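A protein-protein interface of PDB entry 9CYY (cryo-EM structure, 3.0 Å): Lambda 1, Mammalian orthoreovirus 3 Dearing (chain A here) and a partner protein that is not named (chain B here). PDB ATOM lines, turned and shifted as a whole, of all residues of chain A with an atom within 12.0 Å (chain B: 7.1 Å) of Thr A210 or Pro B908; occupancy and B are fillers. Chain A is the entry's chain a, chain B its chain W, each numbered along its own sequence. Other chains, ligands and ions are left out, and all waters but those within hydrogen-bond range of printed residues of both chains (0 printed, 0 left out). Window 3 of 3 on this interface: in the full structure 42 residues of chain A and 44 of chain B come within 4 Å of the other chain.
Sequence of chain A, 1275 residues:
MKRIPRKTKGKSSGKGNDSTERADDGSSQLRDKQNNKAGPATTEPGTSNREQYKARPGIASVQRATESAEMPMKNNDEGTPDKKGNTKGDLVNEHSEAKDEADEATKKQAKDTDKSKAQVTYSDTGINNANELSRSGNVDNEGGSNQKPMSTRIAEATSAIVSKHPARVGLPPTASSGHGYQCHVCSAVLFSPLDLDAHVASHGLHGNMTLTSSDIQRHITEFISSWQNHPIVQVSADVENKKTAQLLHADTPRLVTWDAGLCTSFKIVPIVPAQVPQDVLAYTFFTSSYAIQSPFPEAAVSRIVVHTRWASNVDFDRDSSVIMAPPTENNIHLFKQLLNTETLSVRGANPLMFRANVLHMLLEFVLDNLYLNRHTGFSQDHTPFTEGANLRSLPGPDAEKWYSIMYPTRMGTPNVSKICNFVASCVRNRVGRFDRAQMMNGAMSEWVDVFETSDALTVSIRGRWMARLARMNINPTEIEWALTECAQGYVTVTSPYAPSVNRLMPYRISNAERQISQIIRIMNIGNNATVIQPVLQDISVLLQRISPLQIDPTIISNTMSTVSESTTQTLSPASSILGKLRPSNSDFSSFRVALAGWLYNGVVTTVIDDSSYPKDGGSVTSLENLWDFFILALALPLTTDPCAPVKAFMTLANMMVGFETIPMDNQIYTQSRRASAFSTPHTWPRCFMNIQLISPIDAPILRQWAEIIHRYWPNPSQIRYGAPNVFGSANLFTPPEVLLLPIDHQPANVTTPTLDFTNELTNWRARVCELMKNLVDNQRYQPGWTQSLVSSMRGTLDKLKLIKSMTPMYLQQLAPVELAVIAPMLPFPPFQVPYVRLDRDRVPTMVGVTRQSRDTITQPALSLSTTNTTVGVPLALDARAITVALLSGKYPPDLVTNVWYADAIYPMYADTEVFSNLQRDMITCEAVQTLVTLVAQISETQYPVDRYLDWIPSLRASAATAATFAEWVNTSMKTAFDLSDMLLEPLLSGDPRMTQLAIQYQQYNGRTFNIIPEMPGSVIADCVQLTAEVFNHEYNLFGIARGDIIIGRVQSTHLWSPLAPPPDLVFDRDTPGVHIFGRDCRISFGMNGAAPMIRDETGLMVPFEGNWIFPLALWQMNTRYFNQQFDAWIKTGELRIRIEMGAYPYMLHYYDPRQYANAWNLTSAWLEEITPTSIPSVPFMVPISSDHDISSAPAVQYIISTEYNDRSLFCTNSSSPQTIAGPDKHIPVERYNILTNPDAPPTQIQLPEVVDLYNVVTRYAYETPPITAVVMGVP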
ATOM      1  N   HIS A 203      15.550  12.356 -11.630  1.00  0.00           N
ATOM      2  CA  HIS A 203      16.535  12.120 -12.677  1.00  0.00           C
ATOM      3  C   HIS A 203      17.361  13.372 -12.950  1.00  0.00           C
ATOM      4  O   HIS A 203      16.934  14.256 -13.692  1.00  0.00           O
ATOM      5  CB  HIS A 203      15.852  11.657 -13.965  1.00  0.00           C
ATOM      6  CG  HIS A 203      14.624  10.833 -13.734  1.00  0.00           C
ATOM      7  ND1 HIS A 203      14.645   9.645 -13.037  1.00  0.00           N
ATOM      8  CD2 HIS A 203      13.337  11.026 -14.109  1.00  0.00           C
ATOM      9  CE1 HIS A 203      13.424   9.141 -12.992  1.00  0.00           C
ATOM     10  NE2 HIS A 203      12.612   9.961 -13.636  1.00  0.00           N
ATOM     11  N   GLY A 204      18.545  13.440 -12.349  1.00  0.00           N
ATOM     12  CA  GLY A 204      19.421  14.581 -12.564  1.00  0.00           C
ATOM     13  C   GLY A 204      18.875  15.888 -12.032  1.00  0.00           C
ATOM     14  O   GLY A 204      18.840  16.886 -12.762  1.00  0.00           O
ATOM     15  N   LEU A 205      18.433  15.904 -10.775  1.00  0.00           N
ATOM     16  CA  LEU A 205      17.925  17.116 -10.141  1.00  0.00           C
ATOM     17  C   LEU A 205      18.708  17.512  -8.896  1.00  0.00           C
ATOM     18  O   LEU A 205      18.715  18.689  -8.526  1.00  0.00           O
ATOM     19  CB  LEU A 205      16.443  16.953  -9.778  1.00  0.00           C
ATOM     20  CG  LEU A 205      16.044  16.049  -8.606  1.00  0.00           C
ATOM     21  CD1 LEU A 205      14.609  16.334  -8.200  1.00  0.00           C
ATOM     22  CD2 LEU A 205      16.207  14.574  -8.946  1.00  0.00           C
ATOM     23  N   HIS A 206      19.367  16.559  -8.242  1.00  0.00           N
ATOM     24  CA  HIS A 206      20.100  16.859  -7.020  1.00  0.00           C
ATOM     25  C   HIS A 206      21.352  17.674  -7.324  1.00  0.00           C
ATOM     26  O   HIS A 206      21.738  17.857  -8.481  1.00  0.00           O
ATOM     27  CB  HIS A 206      20.484  15.569  -6.296  1.00  0.00           C
ATOM     28  CG  HIS A 206      19.339  14.902  -5.600  1.00  0.00           C
ATOM     29  ND1 HIS A 206      18.107  14.728  -6.192  1.00  0.00           N
ATOM     30  CD2 HIS A 206      19.241  14.367  -4.361  1.00  0.00           C
ATOM     31  CE1 HIS A 206      17.298  14.115  -5.347  1.00  0.00           C
ATOM     32  NE2 HIS A 206      17.962  13.884  -4.229  1.00  0.00           N
ATOM     33  N   GLY A 207      21.992  18.165  -6.263  1.00  0.00           N
ATOM     34  CA  GLY A 207      23.197  18.957  -6.427  1.00  0.00           C
ATOM     35  C   GLY A 207      24.393  18.168  -6.916  1.00  0.00           C
ATOM     36  O   GLY A 207      25.339  18.759  -7.445  1.00  0.00           O
ATOM     37  N   ASN A 208      24.376  16.844  -6.753  1.00  0.00           N
ATOM     38  CA  ASN A 208      25.495  15.994  -7.161  1.00  0.00           C
ATOM     39  C   ASN A 208      25.345  15.580  -8.629  1.00  0.00           C
ATOM     40  O   ASN A 208      24.805  14.529  -8.979  1.00  0.00           O
ATOM     41  CB  ASN A 208      25.618  14.799  -6.222  1.00  0.00           C
ATOM     42  CG  ASN A 208      24.332  13.999  -6.105  1.00  0.00           C
ATOM     43  OD1 ASN A 208      23.342  14.279  -6.778  1.00  0.00           O
ATOM     44  ND2 ASN A 208      24.345  12.992  -5.238  1.00  0.00           N
ATOM     45  N   MET A 209      25.865  16.439  -9.502  1.00  0.00           N
ATOM     46  CA  MET A 209      25.878  16.213 -10.941  1.00  0.00           C
ATOM     47  C   MET A 209      27.222  15.637 -11.355  1.00  0.00           C
ATOM     48  O   MET A 209      28.264  16.250 -11.106  1.00  0.00           O
ATOM     49  CB  MET A 209      25.627  17.510 -11.714  1.00  0.00           C
ATOM     50  CG  MET A 209      24.259  18.136 -11.527  1.00  0.00           C
ATOM     51  SD  MET A 209      22.924  17.098 -12.146  1.00  0.00           S
ATOM     52  CE  MET A 209      21.508  18.019 -11.563  1.00  0.00           C
ATOM     53  N   THR A 210      27.199  14.474 -11.998  1.00  0.00           N
ATOM     54  CA  THR A 210      28.397  13.862 -12.555  1.00  0.00           C
ATOM     55  C   THR A 210      28.130  13.480 -14.004  1.00  0.00           C
ATOM     56  O   THR A 210      27.253  12.655 -14.280  1.00  0.00           O
ATOM     57  CB  THR A 210      28.819  12.632 -11.750  1.00  0.00           C
ATOM     58  OG1 THR A 210      29.094  13.017 -10.398  1.00  0.00           O
ATOM     59  CG2 THR A 210      30.065  12.005 -12.353  1.00  0.00           C
ATOM     60  N   LEU A 211      28.886  14.079 -14.921  1.00  0.00           N
ATOM     61  CA  LEU A 211      28.706  13.794 -16.338  1.00  0.00           C
ATOM     62  C   LEU A 211      29.147  12.371 -16.653  1.00  0.00           C
ATOM     63  O   LEU A 211      30.160  11.891 -16.139  1.00  0.00           O
ATOM     64  CB  LEU A 211      29.497  14.792 -17.182  1.00  0.00           C
ATOM     65  CG  LEU A 211      29.351  14.654 -18.697  1.00  0.00           C
ATOM     66  CD1 LEU A 211      27.912  14.897 -19.114  1.00  0.00           C
ATOM     67  CD2 LEU A 211      30.289  15.608 -19.415  1.00  0.00           C
ATOM     68  N   THR A 212      28.381  11.694 -17.506  1.00  0.00           N
ATOM     69  CA  THR A 212      28.670  10.307 -17.832  1.00  0.00           C
ATOM     70  C   THR A 212      28.090   9.931 -19.190  1.00  0.00           C
ATOM     71  O   THR A 212      27.215  10.610 -19.745  1.00  0.00           O
ATOM     72  CB  THR A 212      28.140   9.356 -16.751  1.00  0.00           C
ATOM     73  OG1 THR A 212      28.435   8.002 -17.115  1.00  0.00           O
ATOM     74  CG2 THR A 212      26.645   9.525 -16.582  1.00  0.00           C
ATOM     75  N   SER A 213      28.600   8.812 -19.710  1.00  0.00           N
ATOM     76  CA  SER A 213      28.213   8.350 -21.037  1.00  0.00           C
ATOM     77  C   SER A 213      26.734   7.995 -21.095  1.00  0.00           C
ATOM     78  O   SER A 213      26.098   8.149 -22.141  1.00  0.00           O
ATOM     79  CB  SER A 213      29.068   7.150 -21.441  1.00  0.00           C
ATOM     80  OG  SER A 213      28.974   6.114 -20.481  1.00  0.00           O
ATOM     81  N   SER A 214      26.169   7.504 -19.991  1.00  0.00           N
ATOM     82  CA  SER A 214      24.741   7.201 -19.975  1.00  0.00           C
ATOM     83  C   SER A 214      23.915   8.466 -20.170  1.00  0.00           C
ATOM     84  O   SER A 214      22.936   8.476 -20.925  1.00  0.00           O
ATOM     85  CB  SER A 214      24.364   6.500 -18.670  1.00  0.00           C
ATOM     86  OG  SER A 214      24.631   7.322 -17.551  1.00  0.00           O
ATOM     87  N   ASP A 215      24.307   9.553 -19.500  1.00  0.00           N
ATOM     88  CA  ASP A 215      23.632  10.830 -19.704  1.00  0.00           C
ATOM     89  C   ASP A 215      23.802  11.315 -21.137  1.00  0.00           C
ATOM     90  O   ASP A 215      22.858  11.845 -21.741  1.00  0.00           O
ATOM     91  CB  ASP A 215      24.163  11.871 -18.720  1.00  0.00           C
ATOM     92  CG  ASP A 215      23.836  11.532 -17.280  1.00  0.00           C
ATOM     93  OD1 ASP A 215      22.861  10.786 -17.051  1.00  0.00           O
ATOM     94  OD2 ASP A 215      24.548  12.019 -16.377  1.00  0.00           O
ATOM     95  N   ILE A 216      25.003  11.147 -21.695  1.00  0.00           N
ATOM     96  CA  ILE A 216      25.235  11.546 -23.082  1.00  0.00           C
ATOM     97  C   ILE A 216      24.298  10.787 -24.018  1.00  0.00           C
ATOM     98  O   ILE A 216      23.668  11.372 -24.908  1.00  0.00           O
ATOM     99  CB  ILE A 216      26.710  11.327 -23.461  1.00  0.00           C
ATOM    100  CG1 ILE A 216      27.613  12.234 -22.626  1.00  0.00           C
ATOM    101  CG2 ILE A 216      26.924  11.578 -24.941  1.00  0.00           C
ATOM    102  CD1 ILE A 216      29.081  11.913 -22.759  1.00  0.00           C
ATOM    103  N   GLN A 217      24.192   9.472 -23.822  1.00  0.00           N
ATOM    104  CA  GLN A 217      23.323   8.656 -24.663  1.00  0.00           C
ATOM    105  C   GLN A 217      21.864   9.060 -24.508  1.00  0.00           C
ATOM    106  O   GLN A 217      21.119   9.111 -25.494  1.00  0.00           O
ATOM    107  CB  GLN A 217      23.502   7.175 -24.328  1.00  0.00           C
ATOM    108  CG  GLN A 217      24.895   6.634 -24.589  1.00  0.00           C
ATOM    109  CD  GLN A 217      25.240   6.605 -26.060  1.00  0.00           C
ATOM    110  OE1 GLN A 217      24.396   6.300 -26.902  1.00  0.00           O
ATOM    111  NE2 GLN A 217      26.489   6.921 -26.382  1.00  0.00           N
ATOM    112  N   ARG A 218      21.432   9.339 -23.277  1.00  0.00           N
ATOM    113  CA  ARG A 218      20.052   9.758 -23.058  1.00  0.00           C
ATOM    114  C   ARG A 218      19.750  11.051 -23.805  1.00  0.00           C
ATOM    115  O   ARG A 218      18.723  11.165 -24.489  1.00  0.00           O
ATOM    116  CB  ARG A 218      19.791   9.925 -21.562  1.00  0.00           C
ATOM    117  CG  ARG A 218      18.363  10.304 -21.224  1.00  0.00           C
ATOM    118  CD  ARG A 218      18.153  10.387 -19.724  1.00  0.00           C
ATOM    119  NE  ARG A 218      18.942  11.454 -19.118  1.00  0.00           N
ATOM    120  CZ  ARG A 218      19.929  11.257 -18.256  1.00  0.00           C
ATOM    121  NH1 ARG A 218      20.280  10.040 -17.874  1.00  0.00           N
ATOM    122  NH2 ARG A 218      20.579  12.307 -17.763  1.00  0.00           N
ATOM    123  N   HIS A 219      20.648  12.032 -23.698  1.00  0.00           N
ATOM    124  CA  HIS A 219      20.444  13.295 -24.398  1.00  0.00           C
ATOM    125  C   HIS A 219      20.425  13.090 -25.906  1.00  0.00           C
ATOM    126  O   HIS A 219      19.630  13.717 -26.619  1.00  0.00           O
ATOM    127  CB  HIS A 219      21.528  14.295 -24.001  1.00  0.00           C
ATOM    128  CG  HIS A 219      21.501  14.667 -22.552  1.00  0.00           C
ATOM    129  ND1 HIS A 219      20.342  14.676 -21.808  1.00  0.00           N
ATOM    130  CD2 HIS A 219      22.492  15.042 -21.709  1.00  0.00           C
ATOM    131  CE1 HIS A 219      20.618  15.042 -20.570  1.00  0.00           C
ATOM    132  NE2 HIS A 219      21.916  15.269 -20.483  1.00  0.00           N
ATOM    133  N   SER B 883      37.322   9.199 -13.846  1.00  0.00           N
ATOM    134  CA  SER B 883      36.098   9.496 -14.570  1.00  0.00           C
ATOM    135  C   SER B 883      36.056   8.731 -15.889  1.00  0.00           C
ATOM    136  O   SER B 883      37.021   8.079 -16.295  1.00  0.00           O
ATOM    137  CB  SER B 883      35.981  10.995 -14.834  1.00  0.00           C
ATOM    138  OG  SER B 883      36.735  11.366 -15.973  1.00  0.00           O
ATOM    139  N   ILE B 887      35.118  12.603 -22.241  1.00  0.00           N
ATOM    140  CA  ILE B 887      33.917  13.318 -21.832  1.00  0.00           C
ATOM    141  C   ILE B 887      34.126  14.831 -21.858  1.00  0.00           C
ATOM    142  O   ILE B 887      33.361  15.572 -21.252  1.00  0.00           O
ATOM    143  CB  ILE B 887      33.434  12.850 -20.445  1.00  0.00           C
ATOM    144  CG1 ILE B 887      34.461  13.211 -19.370  1.00  0.00           C
ATOM    145  CG2 ILE B 887      33.164  11.355 -20.453  1.00  0.00           C
ATOM    146  CD1 ILE B 887      34.104  12.698 -17.996  1.00  0.00           C
ATOM    147  N   ILE B 903      35.889  21.550 -13.781  1.00  0.00           N
ATOM    148  CA  ILE B 903      35.843  21.257 -12.352  1.00  0.00           C
ATOM    149  C   ILE B 903      34.399  21.107 -11.886  1.00  0.00           C
ATOM    150  O   ILE B 903      34.070  20.194 -11.122  1.00  0.00           O
ATOM    151  CB  ILE B 903      36.588  22.341 -11.554  1.00  0.00           C
ATOM    152  CG1 ILE B 903      38.095  22.212 -11.766  1.00  0.00           C
ATOM    153  CG2 ILE B 903      36.260  22.237 -10.077  1.00  0.00           C
ATOM    154  CD1 ILE B 903      38.889  23.354 -11.181  1.00  0.00           C
ATOM    155  N   SER B 904      33.515  21.998 -12.338  1.00  0.00           N
ATOM    156  CA  SER B 904      32.114  21.898 -11.950  1.00  0.00           C
ATOM    157  C   SER B 904      31.446  20.697 -12.604  1.00  0.00           C
ATOM    158  O   SER B 904      30.525  20.103 -12.032  1.00  0.00           O
ATOM    159  CB  SER B 904      31.379  23.186 -12.312  1.00  0.00           C
ATOM    160  OG  SER B 904      32.075  24.319 -11.827  1.00  0.00           O
ATOM    161  N   LEU B 905      31.890  20.327 -13.808  1.00  0.00           N
ATOM    162  CA  LEU B 905      31.341  19.138 -14.449  1.00  0.00           C
ATOM    163  C   LEU B 905      31.647  17.877 -13.655  1.00  0.00           C
ATOM    164  O   LEU B 905      30.781  17.005 -13.521  1.00  0.00           O
ATOM    165  CB  LEU B 905      31.879  19.007 -15.873  1.00  0.00           C
ATOM    166  CG  LEU B 905      31.182  19.849 -16.942  1.00  0.00           C
ATOM    167  CD1 LEU B 905      31.918  19.745 -18.267  1.00  0.00           C
ATOM    168  CD2 LEU B 905      29.735  19.420 -17.094  1.00  0.00           C
ATOM    169  N   ILE B 906      32.863  17.754 -13.120  1.00  0.00           N
ATOM    170  CA  ILE B 906      33.248  16.536 -12.416  1.00  0.00           C
ATOM    171  C   ILE B 906      33.445  16.759 -10.919  1.00  0.00           C
ATOM    172  O   ILE B 906      34.163  15.995 -10.273  1.00  0.00           O
ATOM    173  CB  ILE B 906      34.501  15.900 -13.050  1.00  0.00           C
ATOM    174  CG1 ILE B 906      35.746  16.745 -12.773  1.00  0.00           C
ATOM    175  CG2 ILE B 906      34.299  15.697 -14.540  1.00  0.00           C
ATOM    176  CD1 ILE B 906      37.030  15.953 -12.794  1.00  0.00           C
ATOM    177  N   ARG B 907      32.787  17.764 -10.341  1.00  0.00           N
ATOM    178  CA  ARG B 907      33.031  18.132  -8.946  1.00  0.00           C
ATOM    179  C   ARG B 907      32.709  17.038  -7.933  1.00  0.00           C
ATOM    180  O   ARG B 907      33.579  16.732  -7.103  1.00  0.00           O
ATOM    181  CB  ARG B 907      32.252  19.415  -8.621  1.00  0.00           C
ATOM    182  CG  ARG B 907      32.860  20.239  -7.501  1.00  0.00           C
ATOM    183  CD  ARG B 907      31.869  21.257  -6.968  1.00  0.00           C
ATOM    184  NE  ARG B 907      30.502  20.750  -6.978  1.00  0.00           N
ATOM    185  CZ  ARG B 907      29.912  20.169  -5.944  1.00  0.00           C
ATOM    186  NH1 ARG B 907      30.541  20.002  -4.792  1.00  0.00           N
ATOM    187  NH2 ARG B 907      28.658  19.742  -6.068  1.00  0.00           N
ATOM    188  N   PRO B 908      31.514  16.428  -7.918  1.00  0.00           N
ATOM    189  CA  PRO B 908      31.226  15.451  -6.852  1.00  0.00           C
ATOM    190  C   PRO B 908      32.156  14.252  -6.859  1.00  0.00           C
ATOM    191  O   PRO B 908      32.474  13.711  -5.792  1.00  0.00           O
ATOM    192  CB  PRO B 908      29.773  15.042  -7.137  1.00  0.00           C
ATOM    193  CG  PRO B 908      29.220  16.150  -7.956  1.00  0.00           C
ATOM    194  CD  PRO B 908      30.357  16.595  -8.811  1.00  0.00           C
ATOM    195  N   LEU B 909      32.603  13.821  -8.038  1.00  0.00           N
ATOM    196  CA  LEU B 909      33.466  12.648  -8.121  1.00  0.00           C
ATOM    197  C   LEU B 909      34.863  12.947  -7.590  1.00  0.00           C
ATOM    198  O   LEU B 909      35.535  12.054  -7.057  1.00  0.00           O
ATOM    199  CB  LEU B 909      33.515  12.156  -9.567  1.00  0.00           C
ATOM    200  CG  LEU B 909      34.281  10.876  -9.888  1.00  0.00           C
ATOM    201  CD1 LEU B 909      33.554  10.088 -10.956  1.00  0.00           C
ATOM    202  CD2 LEU B 909      35.668  11.232 -10.369  1.00  0.00           C
ATOM    203  N   MET B 910      35.318  14.194  -7.731  1.00  0.00           N
ATOM    204  CA  MET B 910      36.643  14.566  -7.247  1.00  0.00           C
ATOM    205  C   MET B 910      36.743  14.405  -5.737  1.00  0.00           C
ATOM    206  O   MET B 910      37.767  13.951  -5.214  1.00  0.00           O
ATOM    207  CB  MET B 910      36.963  16.005  -7.655  1.00  0.00           C
ATOM    208  CG  MET B 910      37.117  16.206  -9.151  1.00  0.00           C
ATOM    209  SD  MET B 910      37.409  17.927  -9.597  1.00  0.00           S
ATOM    210  CE  MET B 910      39.069  18.160  -8.978  1.00  0.00           C
ATOM    211  N   THR B 911      35.686  14.787  -5.018  1.00  0.00           N
ATOM    212  CA  THR B 911      35.687  14.643  -3.566  1.00  0.00           C
ATOM    213  C   THR B 911      35.804  13.179  -3.161  1.00  0.00           C
ATOM    214  O   THR B 911      36.591  12.830  -2.273  1.00  0.00           O
ATOM    215  CB  THR B 911      34.420  15.263  -2.978  1.00  0.00           C
ATOM    216  OG1 THR B 911      34.393  16.664  -3.269  1.00  0.00           O
ATOM    217  CG2 THR B 911      34.379  15.062  -1.473  1.00  0.00           C
ATOM    218  N   ARG B 912      35.033  12.305  -3.812  1.00  0.00           N
ATOM    219  CA  ARG B 912      35.115  10.880  -3.511  1.00  0.00           C
ATOM    220  C   ARG B 912      36.506  10.342  -3.809  1.00  0.00           C
ATOM    221  O   ARG B 912      37.059   9.555  -3.033  1.00  0.00           O
ATOM    222  CB  ARG B 912      34.061  10.105  -4.301  1.00  0.00           C
ATOM    223  CG  ARG B 912      32.714  10.790  -4.406  1.00  0.00           C
ATOM    224  CD  ARG B 912      31.707   9.898  -5.118  1.00  0.00           C
ATOM    225  NE  ARG B 912      31.232   8.814  -4.265  1.00  0.00           N
ATOM    226  CZ  ARG B 912      29.954   8.535  -4.047  1.00  0.00           C
ATOM    227  NH1 ARG B 912      28.987   9.244  -4.605  1.00  0.00           N
ATOM    228  NH2 ARG B 912      29.638   7.518  -3.251  1.00  0.00           N
ATOM    229  N   TRP B 913      37.089  10.757  -4.934  1.00  0.00           N
ATOM    230  CA  TRP B 913      38.418  10.274  -5.296  1.00  0.00           C
ATOM    231  C   TRP B 913      39.457  10.706  -4.267  1.00  0.00           C
ATOM    232  O   TRP B 913      40.296   9.903  -3.841  1.00  0.00           O
ATOM    233  CB  TRP B 913      38.793  10.773  -6.690  1.00  0.00           C
ATOM    234  CG  TRP B 913      40.116  10.268  -7.174  1.00  0.00           C
ATOM    235  CD1 TRP B 913      40.337   9.173  -7.955  1.00  0.00           C
ATOM    236  CD2 TRP B 913      41.402  10.845  -6.918  1.00  0.00           C
ATOM    237  NE1 TRP B 913      41.680   9.027  -8.197  1.00  0.00           N
ATOM    238  CE2 TRP B 913      42.356  10.042  -7.573  1.00  0.00           C
ATOM    239  CE3 TRP B 913      41.839  11.961  -6.199  1.00  0.00           C
ATOM    240  CZ2 TRP B 913      43.719  10.319  -7.530  1.00  0.00           C
ATOM    241  CZ3 TRP B 913      43.193  12.232  -6.156  1.00  0.00           C
ATOM    242  CH2 TRP B 913      44.116  11.416  -6.818  1.00  0.00           C
ATOM    243  N   VAL B 927      32.509  23.608  -1.469  1.00  0.00           N
ATOM    244  CA  VAL B 927      32.768  23.085  -2.803  1.00  0.00           C
ATOM    245  C   VAL B 927      33.215  21.629  -2.765  1.00  0.00           C
ATOM    246  O   VAL B 927      32.707  20.804  -3.525  1.00  0.00           O
ATOM    247  CB  VAL B 927      33.810  23.966  -3.525  1.00  0.00           C
ATOM    248  CG1 VAL B 927      34.194  23.349  -4.857  1.00  0.00           C
ATOM    249  CG2 VAL B 927      33.269  25.369  -3.722  1.00  0.00           C
ATOM    250  N   PHE B 928      34.158  21.292  -1.886  1.00  0.00           N
ATOM    251  CA  PHE B 928      34.742  19.957  -1.855  1.00  0.00           C
ATOM    252  C   PHE B 928      34.415  19.190  -0.581  1.00  0.00           C
ATOM    253  O   PHE B 928      34.917  18.075  -0.401  1.00  0.00           O
ATOM    254  CB  PHE B 928      36.259  20.043  -2.036  1.00  0.00           C
ATOM    255  CG  PHE B 928      36.679  20.449  -3.415  1.00  0.00           C
ATOM    256  CD1 PHE B 928      36.330  19.681  -4.512  1.00  0.00           C
ATOM    257  CD2 PHE B 928      37.419  21.600  -3.618  1.00  0.00           C
ATOM    258  CE1 PHE B 928      36.715  20.052  -5.784  1.00  0.00           C
ATOM    259  CE2 PHE B 928      37.805  21.976  -4.888  1.00  0.00           C
ATOM    260  CZ  PHE B 928      37.454  21.201  -5.973  1.00  0.00           C
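Of the 15 printed residues of chain B, 4 touch a printed residue of chain A.
Hydrophobic or aromatic side chains of chain B that line the printed part of chain A: Pro B908.
Of the 17 printed residues of chain A, 5 touch a printed residue of chain B.
Printed residues of chain A that touch a printed residue of chain B: Gly A207, Asn A208, Met A209, Thr A210 and Leu A211.
Hydrophobic or aromatic side chains of chain A within 4 Å of the printed part of chain B: Leu A211.
Among the printed residues, 7 pairs touch across the chains.
The guanidinium group of Arg B907 is in hydrogen-bond range of the backbone carbonyl oxygen of Val B927.
Gly A207 touches Arg B907.
Asn A208 touches Pro B908.
Leu B905 touches Met A209.
O of Met A209 touches CD of Pro B908 (3.1 Å).
Thr A210 touches Pro B908 (OG1 to CB, 3.9 Å).
O of Ile B887 touches CD2 of Leu A211, at 3.6 Å.
N of Leu A211 touches O of Leu B905, at 3.8 Å.
Of the printed residues of chain B, Gly A207 touches Arg B907.
Of the printed residues of chain B, Met A209 touches Leu B905 and Pro B908.
Of chain B, only Pro B908 comes within 4 Å of Thr A210.
Of the printed residues of chain A, Ile B887 touches Leu A211 (3.6 Å).
Of the printed residues of chain A, Leu B905 touches Met A209 (3.6 Å) and Leu A211 (3.8 Å).
Arg B907 touches just one residue of chain A: Gly A207.
Of chain A, only Asn A208, Met A209 and Thr A210 come within 4 Å of Pro B908.
Met B910 touches none of the printed residues of chain A.
No residue of chain A comes within 4 Å of Arg B912.
The nearest residue of chain B that does not touch Thr A210 is Leu B905 (4.1 Å).
The nearest residue of chain A that does not touch Pro B908 is Gly A207 (4.7 Å).
The nearest printed residue of chain B that does not touch Met A209 is Ser B904 (4.6 Å).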
